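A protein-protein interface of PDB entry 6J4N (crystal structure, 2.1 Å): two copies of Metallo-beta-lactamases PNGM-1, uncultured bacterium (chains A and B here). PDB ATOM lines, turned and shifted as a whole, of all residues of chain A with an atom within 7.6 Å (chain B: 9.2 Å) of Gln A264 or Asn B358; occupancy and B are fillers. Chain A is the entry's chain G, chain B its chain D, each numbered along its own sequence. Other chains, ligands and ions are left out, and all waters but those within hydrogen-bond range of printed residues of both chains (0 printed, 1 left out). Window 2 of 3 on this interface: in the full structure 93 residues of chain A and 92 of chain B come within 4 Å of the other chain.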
ATOM      1  N   PRO A 212     -25.784 -23.905   0.659  1.00  0.00           N
ATOM      2  CA  PRO A 212     -26.938 -24.154   1.523  1.00  0.00           C
ATOM      3  C   PRO A 212     -27.959 -25.000   0.745  1.00  0.00           C
ATOM      4  O   PRO A 212     -28.235 -24.718  -0.411  1.00  0.00           O
ATOM      5  CB  PRO A 212     -27.503 -22.760   1.815  1.00  0.00           C
ATOM      6  CG  PRO A 212     -26.420 -21.782   1.388  1.00  0.00           C
ATOM      7  CD  PRO A 212     -25.660 -22.491   0.279  1.00  0.00           C
ATOM      8  N   ASN A 213     -28.478 -26.042   1.348  1.00  0.00           N
ATOM      9  CA  ASN A 213     -29.489 -26.865   0.639  1.00  0.00           C
ATOM     10  C   ASN A 213     -30.732 -27.107   1.506  1.00  0.00           C
ATOM     11  O   ASN A 213     -30.733 -26.751   2.696  1.00  0.00           O
ATOM     12  CB  ASN A 213     -28.896 -28.200   0.176  1.00  0.00           C
ATOM     13  CG  ASN A 213     -28.473 -29.080   1.329  1.00  0.00           C
ATOM     14  OD1 ASN A 213     -29.309 -29.742   1.923  1.00  0.00           O
ATOM     15  ND2 ASN A 213     -27.169 -29.147   1.613  1.00  0.00           N
ATOM     16  N   ILE A 214     -31.758 -27.709   0.891  1.00  0.00           N
ATOM     17  CA  ILE A 214     -33.089 -27.913   1.538  1.00  0.00           C
ATOM     18  C   ILE A 214     -33.036 -29.151   2.427  1.00  0.00           C
ATOM     19  O   ILE A 214     -33.845 -29.259   3.355  1.00  0.00           O
ATOM     20  CB  ILE A 214     -34.211 -27.991   0.485  1.00  0.00           C
ATOM     21  CG1 ILE A 214     -34.149 -29.257  -0.366  1.00  0.00           C
ATOM     22  CG2 ILE A 214     -34.198 -26.751  -0.390  1.00  0.00           C
ATOM     23  CD1 ILE A 214     -35.200 -29.300  -1.467  1.00  0.00           C
ATOM     24  N   PRO A 217     -31.443 -28.779   6.690  1.00  0.00           N
ATOM     25  CA  PRO A 217     -32.362 -28.227   7.703  1.00  0.00           C
ATOM     26  C   PRO A 217     -33.476 -29.206   8.115  1.00  0.00           C
ATOM     27  O   PRO A 217     -33.833 -29.264   9.291  1.00  0.00           O
ATOM     28  CB  PRO A 217     -32.988 -26.995   7.025  1.00  0.00           C
ATOM     29  CG  PRO A 217     -32.102 -26.699   5.837  1.00  0.00           C
ATOM     30  CD  PRO A 217     -31.503 -28.029   5.426  1.00  0.00           C
ATOM     31  N   SER A 258     -22.348 -19.115   3.175  1.00  0.00           N
ATOM     32  CA  SER A 258     -21.987 -17.875   3.900  1.00  0.00           C
ATOM     33  C   SER A 258     -22.236 -18.058   5.405  1.00  0.00           C
ATOM     34  O   SER A 258     -23.091 -18.906   5.798  1.00  0.00           O
ATOM     35  CB  SER A 258     -22.765 -16.717   3.363  1.00  0.00           C
ATOM     36  OG  SER A 258     -24.119 -16.790   3.833  1.00  0.00           O
ATOM     37  N   ALA A 259     -21.546 -17.267   6.236  1.00  0.00           N
ATOM     38  CA  ALA A 259     -21.841 -17.172   7.694  1.00  0.00           C
ATOM     39  C   ALA A 259     -23.315 -16.810   7.894  1.00  0.00           C
ATOM     40  O   ALA A 259     -23.976 -17.406   8.741  1.00  0.00           O
ATOM     41  CB  ALA A 259     -20.946 -16.148   8.382  1.00  0.00           C
ATOM     42  N   GLN A 260     -23.818 -15.817   7.159  1.00  0.00           N
ATOM     43  CA  GLN A 260     -25.260 -15.445   7.265  1.00  0.00           C
ATOM     44  C   GLN A 260     -26.169 -16.626   6.837  1.00  0.00           C
ATOM     45  O   GLN A 260     -27.158 -16.895   7.541  1.00  0.00           O
ATOM     46  CB  GLN A 260     -25.525 -14.156   6.494  1.00  0.00           C
ATOM     47  CG  GLN A 260     -24.874 -12.932   7.118  1.00  0.00           C
ATOM     48  CD  GLN A 260     -23.468 -12.642   6.644  1.00  0.00           C
ATOM     49  OE1 GLN A 260     -22.866 -13.379   5.860  1.00  0.00           O
ATOM     50  NE2 GLN A 260     -22.944 -11.511   7.099  1.00  0.00           N
ATOM     51  N   SER A 261     -25.844 -17.384   5.788  1.00  0.00           N
ATOM     52  CA  SER A 261     -26.622 -18.610   5.413  1.00  0.00           C
ATOM     53  C   SER A 261     -26.524 -19.675   6.507  1.00  0.00           C
ATOM     54  O   SER A 261     -27.523 -20.336   6.773  1.00  0.00           O
ATOM     55  CB  SER A 261     -26.205 -19.229   4.104  1.00  0.00           C
ATOM     56  OG  SER A 261     -26.447 -18.382   3.002  1.00  0.00           O
ATOM     57  N   PHE A 262     -25.346 -19.884   7.087  1.00  0.00           N
ATOM     58  CA  PHE A 262     -25.152 -20.912   8.136  1.00  0.00           C
ATOM     59  C   PHE A 262     -26.070 -20.560   9.320  1.00  0.00           C
ATOM     60  O   PHE A 262     -26.699 -21.452   9.931  1.00  0.00           O
ATOM     61  CB  PHE A 262     -23.668 -20.985   8.512  1.00  0.00           C
ATOM     62  CG  PHE A 262     -23.395 -21.706   9.798  1.00  0.00           C
ATOM     63  CD1 PHE A 262     -23.799 -21.157  11.006  1.00  0.00           C
ATOM     64  CD2 PHE A 262     -22.769 -22.945   9.794  1.00  0.00           C
ATOM     65  CE1 PHE A 262     -23.604 -21.853  12.181  1.00  0.00           C
ATOM     66  CE2 PHE A 262     -22.535 -23.612  10.980  1.00  0.00           C
ATOM     67  CZ  PHE A 262     -22.945 -23.057  12.167  1.00  0.00           C
ATOM     68  N   GLY A 263     -26.145 -19.265   9.649  1.00  0.00           N
ATOM     69  CA  GLY A 263     -27.104 -18.772  10.667  1.00  0.00           C
ATOM     70  C   GLY A 263     -28.545 -19.130  10.313  1.00  0.00           C
ATOM     71  O   GLY A 263     -29.259 -19.775  11.139  1.00  0.00           O
ATOM     72  N   GLN A 264     -28.972 -18.769   9.105  1.00  0.00           N
ATOM     73  CA  GLN A 264     -30.335 -19.124   8.626  1.00  0.00           C
ATOM     74  C   GLN A 264     -30.549 -20.610   8.874  1.00  0.00           C
ATOM     75  O   GLN A 264     -31.534 -20.952   9.501  1.00  0.00           O
ATOM     76  CB  GLN A 264     -30.590 -18.823   7.145  1.00  0.00           C
ATOM     77  CG  GLN A 264     -31.851 -19.509   6.611  1.00  0.00           C
ATOM     78  CD  GLN A 264     -32.201 -19.144   5.188  1.00  0.00           C
ATOM     79  OE1 GLN A 264     -31.772 -18.118   4.664  1.00  0.00           O
ATOM     80  NE2 GLN A 264     -32.989 -19.992   4.540  1.00  0.00           N
ATOM     81  N   ILE A 265     -29.600 -21.436   8.433  1.00  0.00           N
ATOM     82  CA  ILE A 265     -29.736 -22.920   8.497  1.00  0.00           C
ATOM     83  C   ILE A 265     -29.902 -23.385   9.937  1.00  0.00           C
ATOM     84  O   ILE A 265     -30.791 -24.210  10.166  1.00  0.00           O
ATOM     85  CB  ILE A 265     -28.557 -23.621   7.799  1.00  0.00           C
ATOM     86  CG1 ILE A 265     -28.651 -23.447   6.285  1.00  0.00           C
ATOM     87  CG2 ILE A 265     -28.459 -25.078   8.198  1.00  0.00           C
ATOM     88  CD1 ILE A 265     -27.314 -23.577   5.579  1.00  0.00           C
ATOM     89  N   MET A 266     -29.040 -22.970  10.858  1.00  0.00           N
ATOM     90  CA  MET A 266     -29.125 -23.494  12.258  1.00  0.00           C
ATOM     91  C   MET A 266     -30.312 -22.888  13.029  1.00  0.00           C
ATOM     92  O   MET A 266     -30.800 -23.524  13.998  1.00  0.00           O
ATOM     93  CB  MET A 266     -27.839 -23.186  13.022  1.00  0.00           C
ATOM     94  CG  MET A 266     -26.652 -23.935  12.475  1.00  0.00           C
ATOM     95  SD  MET A 266     -26.779 -25.717  12.713  1.00  0.00           S
ATOM     96  CE  MET A 266     -25.445 -26.172  11.598  1.00  0.00           C
ATOM     97  N   ASN A 267     -30.746 -21.690  12.660  1.00  0.00           N
ATOM     98  CA  ASN A 267     -32.047 -21.151  13.157  1.00  0.00           C
ATOM     99  C   ASN A 267     -33.177 -22.147  12.820  1.00  0.00           C
ATOM    100  O   ASN A 267     -33.918 -22.526  13.743  1.00  0.00           O
ATOM    101  CB  ASN A 267     -32.333 -19.770  12.579  1.00  0.00           C
ATOM    102  CG  ASN A 267     -33.578 -19.145  13.182  1.00  0.00           C
ATOM    103  OD1 ASN A 267     -33.572 -18.675  14.325  1.00  0.00           O
ATOM    104  ND2 ASN A 267     -34.652 -19.129  12.403  1.00  0.00           N
ATOM    105  N   MET A 268     -33.239 -22.629  11.570  1.00  0.00           N
ATOM    106  CA  MET A 268     -34.188 -23.708  11.130  1.00  0.00           C
ATOM    107  C   MET A 268     -33.985 -25.005  11.922  1.00  0.00           C
ATOM    108  O   MET A 268     -34.974 -25.688  12.189  1.00  0.00           O
ATOM    109  CB  MET A 268     -34.056 -24.053   9.639  1.00  0.00           C
ATOM    110  CG  MET A 268     -34.413 -22.903   8.727  1.00  0.00           C
ATOM    111  SD  MET A 268     -33.888 -23.044   6.972  1.00  0.00           S
ATOM    112  CE  MET A 268     -35.238 -23.927   6.193  1.00  0.00           C
ATOM    113  N   VAL A 269     -32.760 -25.382  12.255  1.00  0.00           N
ATOM    114  CA  VAL A 269     -32.498 -26.757  12.776  1.00  0.00           C
ATOM    115  C   VAL A 269     -32.841 -26.816  14.254  1.00  0.00           C
ATOM    116  O   VAL A 269     -33.172 -27.900  14.742  1.00  0.00           O
ATOM    117  CB  VAL A 269     -31.017 -27.113  12.589  1.00  0.00           C
ATOM    118  CG1 VAL A 269     -30.618 -28.343  13.391  1.00  0.00           C
ATOM    119  CG2 VAL A 269     -30.707 -27.292  11.126  1.00  0.00           C
ATOM    120  N   GLN A 270     -32.652 -25.690  14.932  1.00  0.00           N
ATOM    121  CA  GLN A 270     -32.716 -25.572  16.418  1.00  0.00           C
ATOM    122  C   GLN A 270     -31.992 -26.730  17.093  1.00  0.00           C
ATOM    123  O   GLN A 270     -32.602 -27.414  17.906  1.00  0.00           O
ATOM    124  CB  GLN A 270     -34.171 -25.490  16.910  1.00  0.00           C
ATOM    125  CG  GLN A 270     -34.886 -24.215  16.459  1.00  0.00           C
ATOM    126  CD  GLN A 270     -34.289 -22.958  17.053  1.00  0.00           C
ATOM    127  OE1 GLN A 270     -34.119 -22.853  18.262  1.00  0.00           O
ATOM    128  NE2 GLN A 270     -33.949 -21.988  16.214  1.00  0.00           N
ATOM    129  N   GLY A 292     -21.449 -12.542  11.192  1.00  0.00           N
ATOM    130  CA  GLY A 292     -22.309 -13.043  10.094  1.00  0.00           C
ATOM    131  C   GLY A 292     -23.348 -14.043  10.595  1.00  0.00           C
ATOM    132  O   GLY A 292     -24.539 -13.866  10.312  1.00  0.00           O
ATOM    133  N   VAL A 293     -22.918 -15.040  11.357  1.00  0.00           N
ATOM    134  CA  VAL A 293     -23.813 -16.084  11.936  1.00  0.00           C
ATOM    135  C   VAL A 293     -24.838 -15.495  12.919  1.00  0.00           C
ATOM    136  O   VAL A 293     -26.011 -15.998  12.949  1.00  0.00           O
ATOM    137  CB  VAL A 293     -22.996 -17.165  12.654  1.00  0.00           C
ATOM    138  CG1 VAL A 293     -23.898 -18.160  13.350  1.00  0.00           C
ATOM    139  CG2 VAL A 293     -22.076 -17.907  11.703  1.00  0.00           C
ATOM    140  N   GLU A 295     -26.195 -12.625  13.054  1.00  0.00           N
ATOM    141  CA  GLU A 295     -27.289 -11.942  12.298  1.00  0.00           C
ATOM    142  C   GLU A 295     -28.568 -12.802  12.345  1.00  0.00           C
ATOM    143  O   GLU A 295     -29.643 -12.217  12.437  1.00  0.00           O
ATOM    144  CB  GLU A 295     -26.948 -11.679  10.825  1.00  0.00           C
ATOM    145  CG  GLU A 295     -26.052 -10.491  10.545  1.00  0.00           C
ATOM    146  CD  GLU A 295     -25.871 -10.208   9.057  1.00  0.00           C
ATOM    147  OE1 GLU A 295     -24.710 -10.037   8.601  1.00  0.00           O
ATOM    148  OE2 GLU A 295     -26.891 -10.169   8.337  1.00  0.00           O
ATOM    149  N   ASN A 296     -28.485 -14.136  12.282  1.00  0.00           N
ATOM    150  CA  ASN A 296     -29.705 -14.969  12.101  1.00  0.00           C
ATOM    151  C   ASN A 296     -29.824 -16.137  13.073  1.00  0.00           C
ATOM    152  O   ASN A 296     -30.902 -16.750  13.083  1.00  0.00           O
ATOM    153  CB  ASN A 296     -29.784 -15.576  10.708  1.00  0.00           C
ATOM    154  CG  ASN A 296     -29.367 -14.604   9.630  1.00  0.00           C
ATOM    155  OD1 ASN A 296     -29.940 -13.526   9.484  1.00  0.00           O
ATOM    156  ND2 ASN A 296     -28.369 -14.982   8.852  1.00  0.00           N
ATOM    157  N   TYR A 297     -28.789 -16.505  13.820  1.00  0.00           N
ATOM    158  CA  TYR A 297     -28.925 -17.655  14.757  1.00  0.00           C
ATOM    159  C   TYR A 297     -28.376 -17.240  16.107  1.00  0.00           C
ATOM    160  O   TYR A 297     -27.311 -16.632  16.155  1.00  0.00           O
ATOM    161  CB  TYR A 297     -28.239 -18.912  14.214  1.00  0.00           C
ATOM    162  CG  TYR A 297     -28.048 -20.025  15.214  1.00  0.00           C
ATOM    163  CD1 TYR A 297     -29.082 -20.858  15.597  1.00  0.00           C
ATOM    164  CD2 TYR A 297     -26.812 -20.262  15.777  1.00  0.00           C
ATOM    165  CE1 TYR A 297     -28.893 -21.877  16.517  1.00  0.00           C
ATOM    166  CE2 TYR A 297     -26.610 -21.270  16.697  1.00  0.00           C
ATOM    167  CZ  TYR A 297     -27.651 -22.082  17.081  1.00  0.00           C
ATOM    168  OH  TYR A 297     -27.433 -23.078  17.999  1.00  0.00           O
ATOM    169  N   LEU B 353     -28.799 -29.791  -8.271  1.00  0.00           N
ATOM    170  CA  LEU B 353     -28.964 -28.314  -8.369  1.00  0.00           C
ATOM    171  C   LEU B 353     -30.345 -27.905  -7.819  1.00  0.00           C
ATOM    172  O   LEU B 353     -30.423 -26.872  -7.168  1.00  0.00           O
ATOM    173  CB  LEU B 353     -28.700 -27.819  -9.798  1.00  0.00           C
ATOM    174  CG  LEU B 353     -27.243 -28.015 -10.246  1.00  0.00           C
ATOM    175  CD1 LEU B 353     -27.044 -27.639 -11.698  1.00  0.00           C
ATOM    176  CD2 LEU B 353     -26.286 -27.205  -9.373  1.00  0.00           C
ATOM    177  N   ASP B 354     -31.362 -28.750  -7.973  1.00  0.00           N
ATOM    178  CA  ASP B 354     -32.750 -28.505  -7.477  1.00  0.00           C
ATOM    179  C   ASP B 354     -32.837 -28.382  -5.958  1.00  0.00           C
ATOM    180  O   ASP B 354     -33.814 -27.806  -5.483  1.00  0.00           O
ATOM    181  CB  ASP B 354     -33.672 -29.631  -7.925  1.00  0.00           C
ATOM    182  CG  ASP B 354     -34.070 -29.464  -9.375  1.00  0.00           C
ATOM    183  OD1 ASP B 354     -33.852 -28.366  -9.928  1.00  0.00           O
ATOM    184  OD2 ASP B 354     -34.558 -30.435  -9.940  1.00  0.00           O
ATOM    185  N   GLY B 355     -31.876 -28.922  -5.223  1.00  0.00           N
ATOM    186  CA  GLY B 355     -31.872 -28.845  -3.757  1.00  0.00           C
ATOM    187  C   GLY B 355     -31.479 -27.482  -3.205  1.00  0.00           C
ATOM    188  O   GLY B 355     -31.432 -27.393  -2.010  1.00  0.00           O
ATOM    189  N   ARG B 356     -31.145 -26.456  -3.989  1.00  0.00           N
ATOM    190  CA  ARG B 356     -30.522 -25.240  -3.374  1.00  0.00           C
ATOM    191  C   ARG B 356     -31.530 -24.523  -2.465  1.00  0.00           C
ATOM    192  O   ARG B 356     -32.669 -24.329  -2.910  1.00  0.00           O
ATOM    193  CB  ARG B 356     -30.034 -24.226  -4.406  1.00  0.00           C
ATOM    194  CG  ARG B 356     -28.753 -24.586  -5.135  1.00  0.00           C
ATOM    195  CD  ARG B 356     -28.271 -23.385  -5.928  1.00  0.00           C
ATOM    196  NE  ARG B 356     -27.171 -23.781  -6.795  1.00  0.00           N
ATOM    197  CZ  ARG B 356     -25.913 -23.972  -6.394  1.00  0.00           C
ATOM    198  NH1 ARG B 356     -25.573 -23.766  -5.131  1.00  0.00           N
ATOM    199  NH2 ARG B 356     -24.989 -24.366  -7.259  1.00  0.00           N
ATOM    200  N   LEU B 357     -31.125 -24.153  -1.242  1.00  0.00           N
ATOM    201  CA  LEU B 357     -31.964 -23.415  -0.246  1.00  0.00           C
ATOM    202  C   LEU B 357     -32.008 -21.946  -0.650  1.00  0.00           C
ATOM    203  O   LEU B 357     -30.944 -21.369  -0.968  1.00  0.00           O
ATOM    204  CB  LEU B 357     -31.368 -23.542   1.162  1.00  0.00           C
ATOM    205  CG  LEU B 357     -32.172 -22.999   2.358  1.00  0.00           C
ATOM    206  CD1 LEU B 357     -33.525 -23.688   2.511  1.00  0.00           C
ATOM    207  CD2 LEU B 357     -31.379 -23.176   3.655  1.00  0.00           C
ATOM    208  N   ASN B 358     -33.185 -21.335  -0.616  1.00  0.00           N
ATOM    209  CA  ASN B 358     -33.258 -19.869  -0.814  1.00  0.00           C
ATOM    210  C   ASN B 358     -32.693 -19.196   0.433  1.00  0.00           C
ATOM    211  O   ASN B 358     -33.197 -19.483   1.543  1.00  0.00           O
ATOM    212  CB  ASN B 358     -34.665 -19.332  -1.014  1.00  0.00           C
ATOM    213  CG  ASN B 358     -34.600 -17.822  -1.074  1.00  0.00           C
ATOM    214  OD1 ASN B 358     -34.667 -17.145  -0.052  1.00  0.00           O
ATOM    215  ND2 ASN B 358     -34.297 -17.299  -2.248  1.00  0.00           N
ATOM    216  N   VAL B 359     -31.686 -18.345   0.284  1.00  0.00           N
ATOM    217  CA  VAL B 359     -31.103 -17.657   1.476  1.00  0.00           C
ATOM    218  C   VAL B 359     -31.056 -16.148   1.227  1.00  0.00           C
ATOM    219  O   VAL B 359     -30.261 -15.443   1.904  1.00  0.00           O
ATOM    220  CB  VAL B 359     -29.715 -18.241   1.795  1.00  0.00           C
ATOM    221  CG1 VAL B 359     -29.823 -19.638   2.379  1.00  0.00           C
ATOM    222  CG2 VAL B 359     -28.814 -18.252   0.571  1.00  0.00           C
ATOM    223  N   ASP B 360     -31.863 -15.671   0.283  1.00  0.00           N
ATOM    224  CA  ASP B 360     -31.859 -14.244  -0.142  1.00  0.00           C
ATOM    225  C   ASP B 360     -32.046 -13.324   1.078  1.00  0.00           C
ATOM    226  O   ASP B 360     -31.304 -12.331   1.152  1.00  0.00           O
ATOM    227  CB  ASP B 360     -32.922 -13.965  -1.210  1.00  0.00           C
ATOM    228  CG  ASP B 360     -32.649 -14.623  -2.559  1.00  0.00           C
ATOM    229  OD1 ASP B 360     -31.550 -15.173  -2.743  1.00  0.00           O
ATOM    230  OD2 ASP B 360     -33.546 -14.601  -3.422  1.00  0.00           O
ATOM    231  N   GLU B 361     -32.978 -13.630   1.993  1.00  0.00           N
ATOM    232  CA  GLU B 361     -33.362 -12.706   3.107  1.00  0.00           C
ATOM    233  C   GLU B 361     -32.180 -12.554   4.083  1.00  0.00           C
ATOM    234  O   GLU B 361     -31.733 -11.405   4.282  1.00  0.00           O
ATOM    235  CB  GLU B 361     -34.587 -13.169   3.900  1.00  0.00           C
ATOM    236  CG  GLU B 361     -35.897 -13.104   3.142  1.00  0.00           C
ATOM    237  CD  GLU B 361     -36.410 -14.448   2.627  1.00  0.00           C
ATOM    238  OE1 GLU B 361     -37.649 -14.645   2.649  1.00  0.00           O
ATOM    239  OE2 GLU B 361     -35.571 -15.305   2.193  1.00  0.00           O
ATOM    240  N   ALA B 362     -31.746 -13.678   4.671  1.00  0.00           N
ATOM    241  CA  ALA B 362     -30.575 -13.858   5.576  1.00  0.00           C
ATOM    242  C   ALA B 362     -29.308 -13.117   5.091  1.00  0.00           C
ATOM    243  O   ALA B 362     -28.552 -12.627   5.958  1.00  0.00           O
ATOM    244  CB  ALA B 362     -30.310 -15.338   5.711  1.00  0.00           C
ATOM    245  N   ASN B 363     -29.056 -13.061   3.779  1.00  0.00           N
ATOM    246  CA  ASN B 363     -27.816 -12.496   3.175  1.00  0.00           C
ATOM    247  C   ASN B 363     -28.021 -11.059   2.664  1.00  0.00           C
ATOM    248  O   ASN B 363     -27.013 -10.441   2.227  1.00  0.00           O
ATOM    249  CB  ASN B 363     -27.315 -13.382   2.026  1.00  0.00           C
ATOM    250  CG  ASN B 363     -26.650 -14.663   2.499  1.00  0.00           C
ATOM    251  OD1 ASN B 363     -25.432 -14.714   2.618  1.00  0.00           O
ATOM    252  ND2 ASN B 363     -27.426 -15.694   2.798  1.00  0.00           N
ATOM    253  N   ALA B 364     -29.243 -10.518   2.674  1.00  0.00           N
ATOM    254  CA  ALA B 364     -29.525  -9.229   1.986  1.00  0.00           C
ATOM    255  C   ALA B 364     -28.721  -8.099   2.641  1.00  0.00           C
ATOM    256  O   ALA B 364     -28.228  -7.221   1.921  1.00  0.00           O
ATOM    257  CB  ALA B 364     -31.003  -8.921   1.996  1.00  0.00           C
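O of Pro A212 touches CA of Arg B356 (3.8 Å).
CB of Pro A212 touches CG1 of Val B359 (3.9 Å).
Gly B355 touches Asn A213.
O of Asn A213 touches CB of Leu B357, at 3.6 Å.
Ile A214 touches Arg B356 (CG2 to O, 3.8 Å).
Gln A260 touches Ala B362.
Asn B363 touches Gln A260.
Ser A261 touches Val B359.
CA of Val B359 touches OE1 of Gln A264 (3.3 Å).
Leu B357 touches Ile A265 (CD2 to CG1, 3.8 Å).
No residue of chain B comes within 4 Å of Gly A263.
Of chain B, only Leu B357, Asn B358, Val B359 and Ala B362 come within 4 Å of Gln A264.
Tyr A297 touches none of the printed residues of chain B.
Of the printed residues of chain A, Gly B355 touches Asn A213 (3.3 Å) and Ile A214 (2.9 Å).
Asn B358 touches just one residue of chain A: Gln A264.
Of the printed residues of chain A, Val B359 touches Pro A212 (3.9 Å), Ser A261 (3.4 Å) and Gln A264 (3.3 Å).
Asp B360 touches none of the printed residues of chain A.
The nearest residue of chain B that does not touch Gln A264 is Asp B360 (5.0 Å).
The nearest printed residue of chain A that does not touch Asn B363 is Gln A264 (5.3 Å).
No position is printed for both chains.
The side-chain carboxylate (OE1) of Glu A295 is in hydrogen-bond range of the side-chain amide nitrogen (NE2) of Gln A260 (2.7 Å).
The side-chain hydroxyl of Ser A258 sits at hydrogen-bond distance from the backbone NH of Ser A261 (2.7 Å).
ND2 of Asn B358 sits at hydrogen-bond distance from OD2 of Asp B360, at 3.0 Å.
The side-chain amide nitrogen (ND2) of Asn A296 is in hydrogen-bond range of the backbone carbonyl oxygen (O) of Gln A260 (2.6 Å).
The backbone carbonyl oxygen (O) of Val B359 lies within hydrogen-bond range of the side-chain amide nitrogen (ND2) of Asn B363, at 3.0 Å.
The side-chain hydroxyl of Ser A258 lies close to the backbone NH of Gln A260, at 3.5 Å.
Of the 22 printed residues of chain A, 10 touch a printed residue of chain B.
Printed residues of chain A that touch a printed residue of chain B: Pro A212, Asn A213, Ile A214, Ser A258, Gln A260, Ser A261, Gln A264, Ile A265, Glu A295 and Asn A296.
Hydrophobic or aromatic side chains of chain A that line the printed part of chain B: Pro A212, Ile A214 and Ile A265.
Printed residues of chain B that touch a printed residue of chain A: Gly B355, Arg B356, Leu B357, Asn B358, Val B359, Ala B362 and Asn B363.
Hydrophobic or aromatic side chains of chain B within 4 Å of the printed part of chain A: Leu B357, Val B359 and Ala B362.
Among the printed residues, no Asp or Glu carboxylate lies within 4 Å of a Lys or Arg side-chain nitrogen of the other chain.
OD1 of Asn B363 is in hydrogen-bond range of OG of Ser A258 (2.7 Å).
The side-chain hydroxyl of Ser A261 is in hydrogen-bond range of the side-chain amide nitrogen of Asn B363 (2.9 Å).
The backbone carbonyl oxygen of Gly B355 is in hydrogen-bond range of the backbone NH of Ile A214.
The side-chain amide nitrogen (NE2) of Gln A264 lies within hydrogen-bond range of the backbone carbonyl oxygen (O) of Asn B358 (3.0 Å).
The backbone NH of Leu B357 is in hydrogen-bond range of the backbone carbonyl oxygen of Pro A212.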
